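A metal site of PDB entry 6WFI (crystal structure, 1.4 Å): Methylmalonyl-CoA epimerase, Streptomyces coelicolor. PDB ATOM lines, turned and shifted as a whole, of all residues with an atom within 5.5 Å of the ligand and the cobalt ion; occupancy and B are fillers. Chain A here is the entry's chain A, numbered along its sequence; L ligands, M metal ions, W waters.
The indole nitrogen of Trp 74 lies close to a nitrogen (N3) of the ligand (3.5 Å). Merely in contact with the ligand: Asn 36 (3.8 Å), Glu 43 (3.8 Å), Ala 70 (3.5 Å), Val 71 (3.7 Å), Lys 77 (3.99 Å), Leu 107 (3.6 Å), Tyr 108 (3.6 Å), Gly 114 (3.0 Å), Ile 120 (3.7 Å), Phe 122 (3.7 Å), Pro 125 (3.5 Å), Gly 130 (3.3 Å) and Leu 132 (3.5 Å). Hydrophobic or aromatic side chains that line the ligand: His 7, Ala 70, Val 71, Trp 74, His 83, His 84, Leu 107, Ile 120, Phe 122, Pro 125 and Leu 132. Within 4 Å of the ligand: His 7, Asn 36, Gln 39, Glu 43, Gln 60, Ala 70, Val 71, Lys 73, Trp 74, Lys 77, His 83, His 84, Leu 107, Tyr 108, Gly 114, Ser 115, Ile 120, Phe 122, Pro 125, Gly 130, Leu 132 and Glu 134. The nearest printed residue that does not touch the ligand is Val 41 (4.2 Å).
Water W6 lies within hydrogen-bond range of O11 of the ligand (2.5 Å) and NE2 of His 124 (2.9 Å). Water W10 lies within hydrogen-bond range of N1 of the ligand (2.5 Å), N of Leu 132 (3.0 Å) and O of His 83 (3.0 Å). Water W8 bridges O15 of the ligand (2.7 Å) and OH of Tyr 108 (2.8 Å). Water W2 lies within hydrogen-bond range of a ring nitrogen (NE2) of His 83 (2.8 Å) and a nitrogen (N4) of the ligand (2.8 Å). Water W1 lies within hydrogen-bond range of O19 of the ligand, OG of Ser 118 and OE2 of Glu 134. Water W11 bridges the backbone carbonyl oxygen (O) of Ala 70 and an oxygen (O14) of the ligand.
The cobalt ion is bound by a ring nitrogen (NE2) of His 7 (2.2 Å), a ring nitrogen (NE2) of His 84 (2.2 Å), an oxygen (O17) of the ligand (2.2 Å), the side-chain carboxylate (OE1) of Glu 134 (2.2 Å), an oxygen (O18) of the ligand (2.2 Å) and the side-chain amide oxygen (OE1) of Gln 60 (2.3 Å). The cobalt ion has six donor atoms within binding distance.
The backbone NH of Ala 86 is in hydrogen-bond range of the backbone carbonyl oxygen of His 7 (2.9 Å). The side-chain amide nitrogen of Gln 60 sits at hydrogen-bond distance from the side-chain carboxylate of Glu 43, 3.2 Å away. The side-chain hydroxyl (OG) of Ser 115 sits at hydrogen-bond distance from the side-chain carboxylate (OE2) of Glu 43 (2.4 Å). The side-chain amide oxygen of Asn 36 lies within hydrogen-bond range of the backbone NH of Gln 39 (2.9 Å). N of Gly 9 lies within hydrogen-bond range of O of His 84 (2.8 Å). O of Val 41 sits at hydrogen-bond distance from N of Asn 36. The side-chain amide nitrogen (NE2) of Gln 60 is in hydrogen-bond range of the side-chain hydroxyl (OG) of Ser 115, 2.8 Å away. N of His 83 sits at hydrogen-bond distance from O of Gly 9 (2.7 Å).
O19 of the ligand lies within hydrogen-bond range of N of Ser 115 (2.8 Å). N3 of the ligand lies within hydrogen-bond range of O of His 83 (3.0 Å). N3 of the ligand sits close to NE2 of His 83, at 3.4 Å. An oxygen (O9) of the ligand is in salt-bridge range of the side-chain amino group of Lys 73 (3.5 Å). The side-chain hydroxyl (OG) of Ser 115 sits at hydrogen-bond distance from an oxygen (O19) of the ligand (3.1 Å). OE1 of Gln 39 is in hydrogen-bond range of N7 of the ligand (2.9 Å).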
ATOM      1  N   HIS A   7      -8.210   6.256  -9.798  1.00  0.00           N
ATOM      2  CA  HIS A   7      -9.451   6.519 -10.552  1.00  0.00           C
ATOM      3  C   HIS A   7     -10.475   5.476 -10.198  1.00  0.00           C
ATOM      4  O   HIS A   7     -10.223   4.385  -9.673  1.00  0.00           O
ATOM      5  CB  HIS A   7      -9.198   6.560 -12.053  1.00  0.00           C
ATOM      6  CG  HIS A   7      -8.629   5.335 -12.702  1.00  0.00           C
ATOM      7  ND1 HIS A   7      -7.264   5.116 -12.818  1.00  0.00           N
ATOM      8  CD2 HIS A   7      -9.233   4.322 -13.369  1.00  0.00           C
ATOM      9  CE1 HIS A   7      -7.102   3.988 -13.555  1.00  0.00           C
ATOM     10  NE2 HIS A   7      -8.263   3.495 -13.905  1.00  0.00           N
ATOM     11  N   GLY A   9     -13.127   3.326 -12.522  1.00  0.00           N
ATOM     12  CA  GLY A   9     -13.470   2.952 -13.882  1.00  0.00           C
ATOM     13  C   GLY A   9     -14.930   2.696 -14.018  1.00  0.00           C
ATOM     14  O   GLY A   9     -15.480   1.818 -13.293  1.00  0.00           O
ATOM     15  N   ASN A  36      -7.678   2.659 -26.317  1.00  0.00           N
ATOM     16  CA  ASN A  36      -6.711   1.640 -25.973  1.00  0.00           C
ATOM     17  C   ASN A  36      -7.168   0.381 -26.670  1.00  0.00           C
ATOM     18  O   ASN A  36      -8.100  -0.290 -26.220  1.00  0.00           O
ATOM     19  CB  ASN A  36      -6.560   1.469 -24.468  1.00  0.00           C
ATOM     20  CG  ASN A  36      -5.419   0.570 -24.070  1.00  0.00           C
ATOM     21  OD1 ASN A  36      -5.344  -0.524 -24.621  1.00  0.00           O
ATOM     22  ND2 ASN A  36      -4.591   0.998 -23.083  1.00  0.00           N
ATOM     23  N   GLN A  39      -6.829  -3.036 -24.690  1.00  0.00           N
ATOM     24  CA  GLN A  39      -7.854  -3.230 -23.650  1.00  0.00           C
ATOM     25  C   GLN A  39      -9.241  -3.218 -24.259  1.00  0.00           C
ATOM     26  O   GLN A  39     -10.154  -3.728 -23.613  1.00  0.00           O
ATOM     27  CB  GLN A  39      -7.661  -2.152 -22.576  1.00  0.00           C
ATOM     28  CG  GLN A  39      -6.407  -2.312 -21.742  1.00  0.00           C
ATOM     29  CD  GLN A  39      -6.370  -3.581 -20.932  1.00  0.00           C
ATOM     30  OE1 GLN A  39      -7.419  -4.204 -20.620  1.00  0.00           O
ATOM     31  NE2 GLN A  39      -5.150  -3.996 -20.645  1.00  0.00           N
ATOM     32  N   VAL A  41     -11.120  -0.380 -25.286  1.00  0.00           N
ATOM     33  CA  VAL A  41     -11.928   0.740 -24.714  1.00  0.00           C
ATOM     34  C   VAL A  41     -11.629   2.048 -25.398  1.00  0.00           C
ATOM     35  O   VAL A  41     -10.466   2.287 -25.810  1.00  0.00           O
ATOM     36  CB  VAL A  41     -11.681   0.923 -23.198  1.00  0.00           C
ATOM     37  CG1 VAL A  41     -12.156  -0.278 -22.418  1.00  0.00           C
ATOM     38  CG2 VAL A  41     -10.232   1.169 -22.839  1.00  0.00           C
ATOM     39  N   GLU A  43     -11.727   5.724 -23.856  1.00  0.00           N
ATOM     40  CA  GLU A  43     -11.756   6.233 -22.458  1.00  0.00           C
ATOM     41  C   GLU A  43     -11.821   7.719 -22.481  1.00  0.00           C
ATOM     42  O   GLU A  43     -11.218   8.407 -23.365  1.00  0.00           O
ATOM     43  CB  GLU A  43     -10.584   5.709 -21.635  1.00  0.00           C
ATOM     44  CG  GLU A  43      -9.238   6.269 -21.872  1.00  0.00           C
ATOM     45  CD  GLU A  43      -8.202   5.802 -20.818  1.00  0.00           C
ATOM     46  OE1 GLU A  43      -7.536   4.814 -21.108  1.00  0.00           O
ATOM     47  OE2 GLU A  43      -8.110   6.458 -19.767  1.00  0.00           O
ATOM     48  N   GLN A  60     -12.699   7.537 -14.764  1.00  0.00           N
ATOM     49  CA  GLN A  60     -12.334   6.962 -16.068  1.00  0.00           C
ATOM     50  C   GLN A  60     -13.576   6.366 -16.701  1.00  0.00           C
ATOM     51  O   GLN A  60     -14.014   5.279 -16.294  1.00  0.00           O
ATOM     52  CB  GLN A  60     -11.246   5.943 -15.871  1.00  0.00           C
ATOM     53  CG  GLN A  60     -10.754   5.347 -17.159  1.00  0.00           C
ATOM     54  CD  GLN A  60      -9.715   4.325 -16.870  1.00  0.00           C
ATOM     55  OE1 GLN A  60     -10.027   3.227 -16.367  1.00  0.00           O
ATOM     56  NE2 GLN A  60      -8.449   4.700 -17.081  1.00  0.00           N
ATOM     57  N   LEU A  62     -15.524   4.587 -19.721  1.00  0.00           N
ATOM     58  CA  LEU A  62     -15.061   3.591 -20.671  1.00  0.00           C
ATOM     59  C   LEU A  62     -16.230   3.061 -21.483  1.00  0.00           C
ATOM     60  O   LEU A  62     -17.173   2.532 -20.923  1.00  0.00           O
ATOM     61  CB  LEU A  62     -14.440   2.405 -19.924  1.00  0.00           C
ATOM     62  CG  LEU A  62     -13.265   2.813 -19.063  1.00  0.00           C
ATOM     63  CD1 LEU A  62     -13.157   1.877 -17.883  1.00  0.00           C
ATOM     64  CD2 LEU A  62     -12.002   2.947 -19.883  1.00  0.00           C
ATOM     65  N   ALA A  70     -13.083  -6.936 -22.145  1.00  0.00           N
ATOM     66  CA  ALA A  70     -13.475  -6.956 -20.737  1.00  0.00           C
ATOM     67  C   ALA A  70     -14.712  -6.082 -20.530  1.00  0.00           C
ATOM     68  O   ALA A  70     -15.699  -6.480 -19.879  1.00  0.00           O
ATOM     69  CB  ALA A  70     -12.303  -6.512 -19.887  1.00  0.00           C
ATOM     70  N   VAL A  71     -14.700  -4.835 -20.991  1.00  0.00           N
ATOM     71  CA  VAL A  71     -15.832  -3.928 -20.725  1.00  0.00           C
ATOM     72  C   VAL A  71     -17.079  -4.341 -21.540  1.00  0.00           C
ATOM     73  O   VAL A  71     -18.182  -4.198 -21.061  1.00  0.00           O
ATOM     74  CB  VAL A  71     -15.438  -2.445 -20.918  1.00  0.00           C
ATOM     75  CG1 VAL A  71     -16.583  -1.516 -20.754  1.00  0.00           C
ATOM     76  CG2 VAL A  71     -14.306  -2.119 -19.949  1.00  0.00           C
ATOM     77  N   LYS A  73     -18.031  -7.314 -22.453  1.00  0.00           N
ATOM     78  CA  LYS A  73     -18.685  -8.470 -21.810  1.00  0.00           C
ATOM     79  C   LYS A  73     -19.360  -8.011 -20.542  1.00  0.00           C
ATOM     80  O   LYS A  73     -20.451  -8.452 -20.154  1.00  0.00           O
ATOM     81  CB  LYS A  73     -17.656  -9.521 -21.427  1.00  0.00           C
ATOM     82  CG  LYS A  73     -17.124 -10.342 -22.574  1.00  0.00           C
ATOM     83  CD  LYS A  73     -16.251 -11.484 -22.033  1.00  0.00           C
ATOM     84  CE  LYS A  73     -16.885 -12.199 -20.859  1.00  0.00           C
ATOM     85  NZ  LYS A  73     -16.327 -13.559 -20.634  1.00  0.00           N
ATOM     86  N   TRP A  74     -18.684  -7.150 -19.773  1.00  0.00           N
ATOM     87  CA  TRP A  74     -19.222  -6.746 -18.495  1.00  0.00           C
ATOM     88  C   TRP A  74     -20.505  -5.947 -18.693  1.00  0.00           C
ATOM     89  O   TRP A  74     -21.479  -6.132 -17.967  1.00  0.00           O
ATOM     90  CB  TRP A  74     -18.104  -6.012 -17.738  1.00  0.00           C
ATOM     91  CG  TRP A  74     -18.473  -5.752 -16.346  1.00  0.00           C
ATOM     92  CD1 TRP A  74     -18.243  -6.531 -15.265  1.00  0.00           C
ATOM     93  CD2 TRP A  74     -19.204  -4.630 -15.924  1.00  0.00           C
ATOM     94  NE1 TRP A  74     -18.754  -5.949 -14.176  1.00  0.00           N
ATOM     95  CE2 TRP A  74     -19.348  -4.775 -14.525  1.00  0.00           C
ATOM     96  CE3 TRP A  74     -19.721  -3.480 -16.531  1.00  0.00           C
ATOM     97  CZ2 TRP A  74     -19.985  -3.839 -13.761  1.00  0.00           C
ATOM     98  CZ3 TRP A  74     -20.364  -2.568 -15.770  1.00  0.00           C
ATOM     99  CH2 TRP A  74     -20.476  -2.721 -14.422  1.00  0.00           C
ATOM    100  N   LYS A  77     -23.534  -8.081 -19.558  1.00  0.00           N
ATOM    101  CA  LYS A  77     -24.035  -8.852 -18.388  1.00  0.00           C
ATOM    102  C   LYS A  77     -24.690  -7.926 -17.384  1.00  0.00           C
ATOM    103  O   LYS A  77     -25.697  -8.319 -16.801  1.00  0.00           O
ATOM    104  CB  LYS A  77     -22.983  -9.635 -17.609  1.00  0.00           C
ATOM    105  CG  LYS A  77     -23.419 -10.059 -16.195  1.00  0.00           C
ATOM    106  CD  LYS A  77     -22.510 -11.011 -15.443  1.00  0.00           C
ATOM    107  CE  LYS A  77     -22.978 -11.327 -14.033  1.00  0.00           C
ATOM    108  NZ  LYS A  77     -22.568 -10.306 -13.049  1.00  0.00           N
ATOM    109  N   HIS A  83     -17.121  -0.361 -12.959  1.00  0.00           N
ATOM    110  CA  HIS A  83     -16.447  -1.548 -13.462  1.00  0.00           C
ATOM    111  C   HIS A  83     -15.215  -1.908 -12.644  1.00  0.00           C
ATOM    112  O   HIS A  83     -14.966  -3.094 -12.421  1.00  0.00           O
ATOM    113  CB  HIS A  83     -16.085  -1.333 -14.929  1.00  0.00           C
ATOM    114  CG  HIS A  83     -15.309  -2.450 -15.538  1.00  0.00           C
ATOM    115  ND1 HIS A  83     -13.943  -2.319 -15.753  1.00  0.00           N
ATOM    116  CD2 HIS A  83     -15.643  -3.737 -15.859  1.00  0.00           C
ATOM    117  CE1 HIS A  83     -13.474  -3.462 -16.212  1.00  0.00           C
ATOM    118  NE2 HIS A  83     -14.508  -4.344 -16.350  1.00  0.00           N
ATOM    119  N   HIS A  84     -14.418  -0.950 -12.193  1.00  0.00           N
ATOM    120  CA  HIS A  84     -13.203  -1.257 -11.420  1.00  0.00           C
ATOM    121  C   HIS A  84     -12.791  -0.058 -10.596  1.00  0.00           C
ATOM    122  O   HIS A  84     -13.297   1.066 -10.837  1.00  0.00           O
ATOM    123  CB  HIS A  84     -12.051  -1.742 -12.311  1.00  0.00           C
ATOM    124  CG  HIS A  84     -11.507  -0.736 -13.276  1.00  0.00           C
ATOM    125  ND1 HIS A  84     -12.018  -0.632 -14.555  1.00  0.00           N
ATOM    126  CD2 HIS A  84     -10.436   0.095 -13.214  1.00  0.00           C
ATOM    127  CE1 HIS A  84     -11.241   0.288 -15.193  1.00  0.00           C
ATOM    128  NE2 HIS A  84     -10.276   0.741 -14.425  1.00  0.00           N
ATOM    129  N   ALA A  86      -9.038   1.815  -9.131  1.00  0.00           N
ATOM    130  CA  ALA A  86      -7.594   1.859  -9.347  1.00  0.00           C
ATOM    131  C   ALA A  86      -6.856   2.582  -8.262  1.00  0.00           C
ATOM    132  O   ALA A  86      -7.258   3.696  -7.905  1.00  0.00           O
ATOM    133  CB  ALA A  86      -7.289   2.483 -10.679  1.00  0.00           C
ATOM    134  N   LEU A 107      -3.148 -10.318 -12.864  1.00  0.00           N
ATOM    135  CA  LEU A 107      -3.503 -10.740 -14.201  1.00  0.00           C
ATOM    136  C   LEU A 107      -2.332 -10.588 -15.183  1.00  0.00           C
ATOM    137  O   LEU A 107      -2.326 -11.452 -16.096  1.00  0.00           O
ATOM    138  CB  LEU A 107      -4.759  -9.996 -14.669  1.00  0.00           C
ATOM    139  CG  LEU A 107      -6.008 -10.162 -13.828  1.00  0.00           C
ATOM    140  CD1 LEU A 107      -7.208  -9.568 -14.563  1.00  0.00           C
ATOM    141  CD2 LEU A 107      -6.349 -11.550 -13.344  1.00  0.00           C
ATOM    142  N   TYR A 108      -1.434  -9.657 -15.018  1.00  0.00           N
ATOM    143  CA  TYR A 108      -0.350  -9.541 -16.041  1.00  0.00           C
ATOM    144  C   TYR A 108       0.952 -10.037 -15.458  1.00  0.00           C
ATOM    145  O   TYR A 108       1.311  -9.692 -14.384  1.00  0.00           O
ATOM    146  CB  TYR A 108      -0.334  -8.090 -16.585  1.00  0.00           C
ATOM    147  CG  TYR A 108      -1.631  -7.638 -17.193  1.00  0.00           C
ATOM    148  CD1 TYR A 108      -2.508  -8.487 -17.820  1.00  0.00           C
ATOM    149  CD2 TYR A 108      -2.015  -6.311 -17.172  1.00  0.00           C
ATOM    150  CE1 TYR A 108      -3.710  -8.069 -18.352  1.00  0.00           C
ATOM    151  CE2 TYR A 108      -3.226  -5.887 -17.652  1.00  0.00           C
ATOM    152  CZ  TYR A 108      -4.096  -6.740 -18.258  1.00  0.00           C
ATOM    153  OH  TYR A 108      -5.289  -6.296 -18.729  1.00  0.00           O
ATOM    154  N   ARG A 113       0.336  -1.037 -20.860  1.00  0.00           N
ATOM    155  CA  ARG A 113       0.056   0.402 -21.009  1.00  0.00           C
ATOM    156  C   ARG A 113      -1.385   0.732 -20.704  1.00  0.00           C
ATOM    157  O   ARG A 113      -2.317   0.122 -21.243  1.00  0.00           O
ATOM    158  CB  ARG A 113       0.322   0.854 -22.465  1.00  0.00           C
ATOM    159  CG  ARG A 113       0.138   2.356 -22.666  1.00  0.00           C
ATOM    160  CD  ARG A 113       0.765   2.916 -23.952  1.00  0.00           C
ATOM    161  NE  ARG A 113       0.245   2.275 -25.136  1.00  0.00           N
ATOM    162  CZ  ARG A 113      -0.893   2.561 -25.727  1.00  0.00           C
ATOM    163  NH1 ARG A 113      -1.680   3.520 -25.287  1.00  0.00           N
ATOM    164  NH2 ARG A 113      -1.182   1.954 -26.861  1.00  0.00           N
ATOM    165  N   GLY A 114      -1.582   1.770 -19.912  1.00  0.00           N
ATOM    166  CA  GLY A 114      -2.884   2.338 -19.676  1.00  0.00           C
ATOM    167  C   GLY A 114      -2.900   3.819 -19.996  1.00  0.00           C
ATOM    168  O   GLY A 114      -2.012   4.311 -20.714  1.00  0.00           O
ATOM    169  N   SER A 115      -3.807   4.514 -19.365  1.00  0.00           N
ATOM    170  CA  SER A 115      -4.136   5.923 -19.681  1.00  0.00           C
ATOM    171  C   SER A 115      -2.876   6.773 -19.616  1.00  0.00           C
ATOM    172  O   SER A 115      -2.109   6.687 -18.680  1.00  0.00           O
ATOM    173  CB  SER A 115      -5.094   6.479 -18.678  1.00  0.00           C
ATOM    174  OG  SER A 115      -6.196   5.612 -18.501  1.00  0.00           O
ATOM    175  N   SER A 118       0.574   5.491 -18.695  1.00  0.00           N
ATOM    176  CA  SER A 118       0.718   4.830 -17.373  1.00  0.00           C
ATOM    177  C   SER A 118       1.004   3.332 -17.615  1.00  0.00           C
ATOM    178  O   SER A 118       0.758   2.763 -18.668  1.00  0.00           O
ATOM    179  CB  SER A 118      -0.507   5.056 -16.509  1.00  0.00           C
ATOM    180  OG  SER A 118      -1.660   4.482 -17.071  1.00  0.00           O
ATOM    181  N   ILE A 120       0.076  -0.362 -15.874  1.00  0.00           N
ATOM    182  CA  ILE A 120      -1.070  -0.824 -15.081  1.00  0.00           C
ATOM    183  C   ILE A 120      -1.010  -2.344 -14.958  1.00  0.00           C
ATOM    184  O   ILE A 120      -0.542  -3.093 -15.871  1.00  0.00           O
ATOM    185  CB  ILE A 120      -2.410  -0.401 -15.720  1.00  0.00           C
ATOM    186  CG1 ILE A 120      -2.760  -1.114 -17.025  1.00  0.00           C
ATOM    187  CG2 ILE A 120      -2.439   1.119 -15.888  1.00  0.00           C
ATOM    188  CD1 ILE A 120      -4.117  -0.760 -17.600  1.00  0.00           C
ATOM    189  N   PHE A 122      -3.847  -5.571 -13.020  1.00  0.00           N
ATOM    190  CA  PHE A 122      -5.127  -5.843 -12.363  1.00  0.00           C
ATOM    191  C   PHE A 122      -5.040  -7.025 -11.436  1.00  0.00           C
ATOM    192  O   PHE A 122      -4.195  -7.944 -11.704  1.00  0.00           O
ATOM    193  CB  PHE A 122      -6.218  -6.122 -13.370  1.00  0.00           C
ATOM    194  CG  PHE A 122      -6.587  -4.923 -14.208  1.00  0.00           C
ATOM    195  CD1 PHE A 122      -7.607  -4.066 -13.818  1.00  0.00           C
ATOM    196  CD2 PHE A 122      -5.991  -4.709 -15.417  1.00  0.00           C
ATOM    197  CE1 PHE A 122      -7.941  -2.952 -14.619  1.00  0.00           C
ATOM    198  CE2 PHE A 122      -6.342  -3.636 -16.202  1.00  0.00           C
ATOM    199  CZ  PHE A 122      -7.303  -2.798 -15.816  1.00  0.00           C
ATOM    200  N   HIS A 124      -7.463 -10.061  -9.635  1.00  0.00           N
ATOM    201  CA  HIS A 124      -8.695 -10.746 -10.011  1.00  0.00           C
ATOM    202  C   HIS A 124      -9.790 -10.424  -9.006  1.00  0.00           C
ATOM    203  O   HIS A 124      -9.596 -10.499  -7.793  1.00  0.00           O
ATOM    204  CB  HIS A 124      -8.465 -12.287  -9.992  1.00  0.00           C
ATOM    205  CG  HIS A 124      -9.516 -13.015 -10.737  1.00  0.00           C
ATOM    206  ND1 HIS A 124     -10.808 -13.057 -10.316  1.00  0.00           N
ATOM    207  CD2 HIS A 124      -9.425 -13.689 -11.926  1.00  0.00           C
ATOM    208  CE1 HIS A 124     -11.497 -13.766 -11.246  1.00  0.00           C
ATOM    209  NE2 HIS A 124     -10.691 -14.158 -12.202  1.00  0.00           N
ATOM    210  N   PRO A 125     -10.993 -10.034  -9.491  1.00  0.00           N
ATOM    211  CA  PRO A 125     -12.029  -9.624  -8.569  1.00  0.00           C
ATOM    212  C   PRO A 125     -12.458 -10.677  -7.590  1.00  0.00           C
ATOM    213  O   PRO A 125     -12.877 -10.400  -6.480  1.00  0.00           O
ATOM    214  CB  PRO A 125     -13.192  -9.219  -9.483  1.00  0.00           C
ATOM    215  CG  PRO A 125     -12.892  -9.887 -10.804  1.00  0.00           C
ATOM    216  CD  PRO A 125     -11.394  -9.940 -10.891  1.00  0.00           C
ATOM    217  N   LYS A 126     -12.313 -11.958  -7.998  1.00  0.00           N
ATOM    218  CA  LYS A 126     -12.765 -13.027  -7.077  1.00  0.00           C
ATOM    219  C   LYS A 126     -11.752 -13.188  -5.950  1.00  0.00           C
ATOM    220  O   LYS A 126     -12.129 -13.809  -4.916  1.00  0.00           O
ATOM    221  CB  LYS A 126     -12.991 -14.339  -7.853  1.00  0.00           C
ATOM    222  CG  LYS A 126     -14.183 -14.297  -8.776  1.00  0.00           C
ATOM    223  CD  LYS A 126     -15.485 -14.283  -8.022  1.00  0.00           C
ATOM    224  CE  LYS A 126     -15.732 -15.611  -7.327  1.00  0.00           C
ATOM    225  NZ  LYS A 126     -15.180 -16.743  -8.099  1.00  0.00           N
ATOM    226  N   GLY A 130     -14.874  -9.252  -4.766  1.00  0.00           N
ATOM    227  CA  GLY A 130     -15.755  -8.850  -5.828  1.00  0.00           C
ATOM    228  C   GLY A 130     -15.390  -7.539  -6.543  1.00  0.00           C
ATOM    229  O   GLY A 130     -16.182  -7.115  -7.337  1.00  0.00           O
ATOM    230  N   VAL A 131     -14.235  -6.960  -6.202  1.00  0.00           N
ATOM    231  CA  VAL A 131     -13.837  -5.648  -6.794  1.00  0.00           C
ATOM    232  C   VAL A 131     -12.669  -5.879  -7.717  1.00  0.00           C
ATOM    233  O   VAL A 131     -11.560  -6.270  -7.297  1.00  0.00           O
ATOM    234  CB  VAL A 131     -13.511  -4.662  -5.683  1.00  0.00           C
ATOM    235  CG1 VAL A 131     -13.029  -3.334  -6.304  1.00  0.00           C
ATOM    236  CG2 VAL A 131     -14.700  -4.438  -4.768  1.00  0.00           C
ATOM    237  N   LEU A 132     -12.869  -5.640  -9.014  1.00  0.00           N
ATOM    238  CA  LEU A 132     -11.776  -5.614  -9.977  1.00  0.00           C
ATOM    239  C   LEU A 132     -10.874  -4.437  -9.622  1.00  0.00           C
ATOM    240  O   LEU A 132     -11.372  -3.299  -9.587  1.00  0.00           O
ATOM    241  CB  LEU A 132     -12.265  -5.548 -11.411  1.00  0.00           C
ATOM    242  CG  LEU A 132     -11.195  -5.385 -12.473  1.00  0.00           C
ATOM    243  CD1 LEU A 132     -10.225  -6.553 -12.508  1.00  0.00           C
ATOM    244  CD2 LEU A 132     -11.841  -5.222 -13.829  1.00  0.00           C
ATOM    245  N   GLU A 134      -7.287  -2.310 -10.019  1.00  0.00           N
ATOM    246  CA  GLU A 134      -6.129  -1.956 -10.839  1.00  0.00           C
ATOM    247  C   GLU A 134      -5.095  -1.271  -9.967  1.00  0.00           C
ATOM    248  O   GLU A 134      -5.409  -0.549  -9.030  1.00  0.00           O
ATOM    249  CB  GLU A 134      -6.563  -1.017 -11.947  1.00  0.00           C
ATOM    250  CG  GLU A 134      -5.461  -0.429 -12.765  1.00  0.00           C
ATOM    251  CD  GLU A 134      -5.979   0.640 -13.692  1.00  0.00           C
ATOM    252  OE1 GLU A 134      -7.186   0.644 -14.007  1.00  0.00           O
ATOM    253  OE2 GLU A 134      -5.154   1.509 -14.131  1.00  0.00           O
HETATM  254  N1  LIG L   1     -15.845  -6.756 -11.326  1.00  0.00           N
HETATM  255  C1  LIG L   1     -16.225  -7.811 -10.556  1.00  0.00           C
HETATM  256  N2  LIG L   1     -16.321  -9.008 -10.937  1.00  0.00           N
HETATM  257  C2  LIG L   1     -16.131  -9.271 -12.198  1.00  0.00           C
HETATM  258  C3  LIG L   1     -15.805  -8.269 -13.139  1.00  0.00           C
HETATM  259  C4  LIG L   1     -15.675  -6.911 -12.667  1.00  0.00           C
HETATM  260  N3  LIG L   1     -15.330  -5.875 -13.463  1.00  0.00           N
HETATM  261  N4  LIG L   1     -15.679  -8.766 -14.408  1.00  0.00           N
HETATM  262  C5  LIG L   1     -15.933 -10.117 -14.191  1.00  0.00           C
HETATM  263  N5  LIG L   1     -16.205 -10.366 -12.940  1.00  0.00           N
HETATM  264  C6  LIG L   1     -16.583 -11.717 -12.392  1.00  0.00           C
HETATM  265  C7  LIG L   1     -17.724 -12.385 -13.166  1.00  0.00           C
HETATM  266  O1  LIG L   1     -18.945 -11.930 -12.673  1.00  0.00           O
HETATM  267  C8  LIG L   1     -17.472 -13.875 -12.976  1.00  0.00           C
HETATM  268  O2  LIG L   1     -18.035 -14.108 -11.744  1.00  0.00           O
HETATM  269  C9  LIG L   1     -15.962 -13.940 -12.910  1.00  0.00           C
HETATM  270  O3  LIG L   1     -15.494 -12.536 -12.687  1.00  0.00           O
HETATM  271  C10 LIG L   1     -15.393 -14.344 -14.232  1.00  0.00           C
HETATM  272  O4  LIG L   1     -16.024 -13.503 -15.222  1.00  0.00           O
HETATM  273  O5  LIG L   1     -20.247 -15.071 -12.494  1.00  0.00           O
HETATM  274  P1  LIG L   1     -19.092 -15.434 -11.569  1.00  0.00           P
HETATM  275  O6  LIG L   1     -18.200 -16.485 -12.155  1.00  0.00           O
HETATM  276  O7  LIG L   1     -19.217 -15.399 -10.071  1.00  0.00           O
HETATM  277  P2  LIG L   1     -15.996 -13.608 -16.828  1.00  0.00           P
HETATM  278  O8  LIG L   1     -15.868 -15.082 -17.151  1.00  0.00           O
HETATM  279  O9  LIG L   1     -17.289 -12.927 -17.302  1.00  0.00           O
HETATM  280  O10 LIG L   1     -14.827 -12.780 -17.507  1.00  0.00           O
HETATM  281  P3  LIG L   1     -13.309 -13.357 -17.399  1.00  0.00           P
HETATM  282  O11 LIG L   1     -13.145 -14.277 -16.235  1.00  0.00           O
HETATM  283  O12 LIG L   1     -12.826 -13.774 -18.772  1.00  0.00           O
HETATM  284  O13 LIG L   1     -12.664 -11.866 -17.222  1.00  0.00           O
HETATM  285  C11 LIG L   1     -12.751 -11.266 -15.900  1.00  0.00           C
HETATM  286  C12 LIG L   1     -11.495 -10.438 -15.795  1.00  0.00           C
HETATM  287  C13 LIG L   1     -10.867 -10.121 -14.476  1.00  0.00           C
HETATM  288  C14 LIG L   1     -10.412 -11.525 -16.116  1.00  0.00           C
HETATM  289  C15 LIG L   1     -11.256  -9.650 -16.998  1.00  0.00           C
HETATM  290  O14 LIG L   1     -12.312  -8.794 -17.250  1.00  0.00           O
HETATM  291  C16 LIG L   1     -10.054  -8.780 -17.082  1.00  0.00           C
HETATM  292  O15 LIG L   1      -9.053  -9.221 -17.619  1.00  0.00           O
HETATM  293  N6  LIG L   1     -10.027  -7.548 -16.608  1.00  0.00           N
HETATM  294  C17 LIG L   1      -8.844  -6.675 -16.681  1.00  0.00           C
HETATM  295  C18 LIG L   1      -8.747  -5.791 -17.911  1.00  0.00           C
HETATM  296  C19 LIG L   1      -9.818  -4.744 -17.940  1.00  0.00           C
HETATM  297  O16 LIG L   1     -10.785  -4.726 -17.173  1.00  0.00           O
HETATM  298  N7  LIG L   1      -9.739  -3.855 -18.918  1.00  0.00           N
HETATM  299  C20 LIG L   1     -10.708  -2.763 -19.116  1.00  0.00           C
HETATM  300  C21 LIG L   1     -10.178  -1.494 -18.336  1.00  0.00           C
HETATM  301  S1  LIG L   1      -8.890  -0.725 -19.308  1.00  0.00           S
HETATM  302  C22 LIG L   1      -8.288   0.428 -18.115  1.00  0.00           C
HETATM  303  O17 LIG L   1      -8.775   0.472 -16.984  1.00  0.00           O
HETATM  304  C23 LIG L   1      -7.183   1.286 -18.526  1.00  0.00           C
HETATM  305  C24 LIG L   1      -6.764   1.304 -19.991  1.00  0.00           C
HETATM  306  N8  LIG L   1      -6.535   2.029 -17.744  1.00  0.00           N
HETATM  307  O18 LIG L   1      -6.856   2.391 -16.543  1.00  0.00           O
HETATM  308  O19 LIG L   1      -5.459   2.606 -18.122  1.00  0.00           O
HETATM  309 CO    CO M   1      -8.565   1.812 -15.264  1.00  0.00          CO
HETATM  310  O   HOH W   1      -4.344   4.041 -15.790  1.00  0.00           O
HETATM  311  O   HOH W   2     -14.531  -7.130 -16.434  1.00  0.00           O
HETATM  312  O   HOH W   3     -19.346  -6.710 -11.097  1.00  0.00           O
HETATM  313  O   HOH W   4      -9.013 -14.674 -15.904  1.00  0.00           O
HETATM  314  O   HOH W   5     -18.153  -9.887 -17.208  1.00  0.00           O
HETATM  315  O   HOH W   6     -11.599 -15.382 -14.660  1.00  0.00           O
HETATM  316  O   HOH W   7     -19.705  -9.085 -10.099  1.00  0.00           O
HETATM  317  O   HOH W   8      -7.058  -8.410 -19.258  1.00  0.00           O
HETATM  318  O   HOH W   9     -10.521 -13.245 -19.853  1.00  0.00           O
HETATM  319  O   HOH W  10     -15.511  -4.656  -9.928  1.00  0.00           O
HETATM  320  O   HOH W  11     -15.522  -8.841 -18.640  1.00  0.00           O
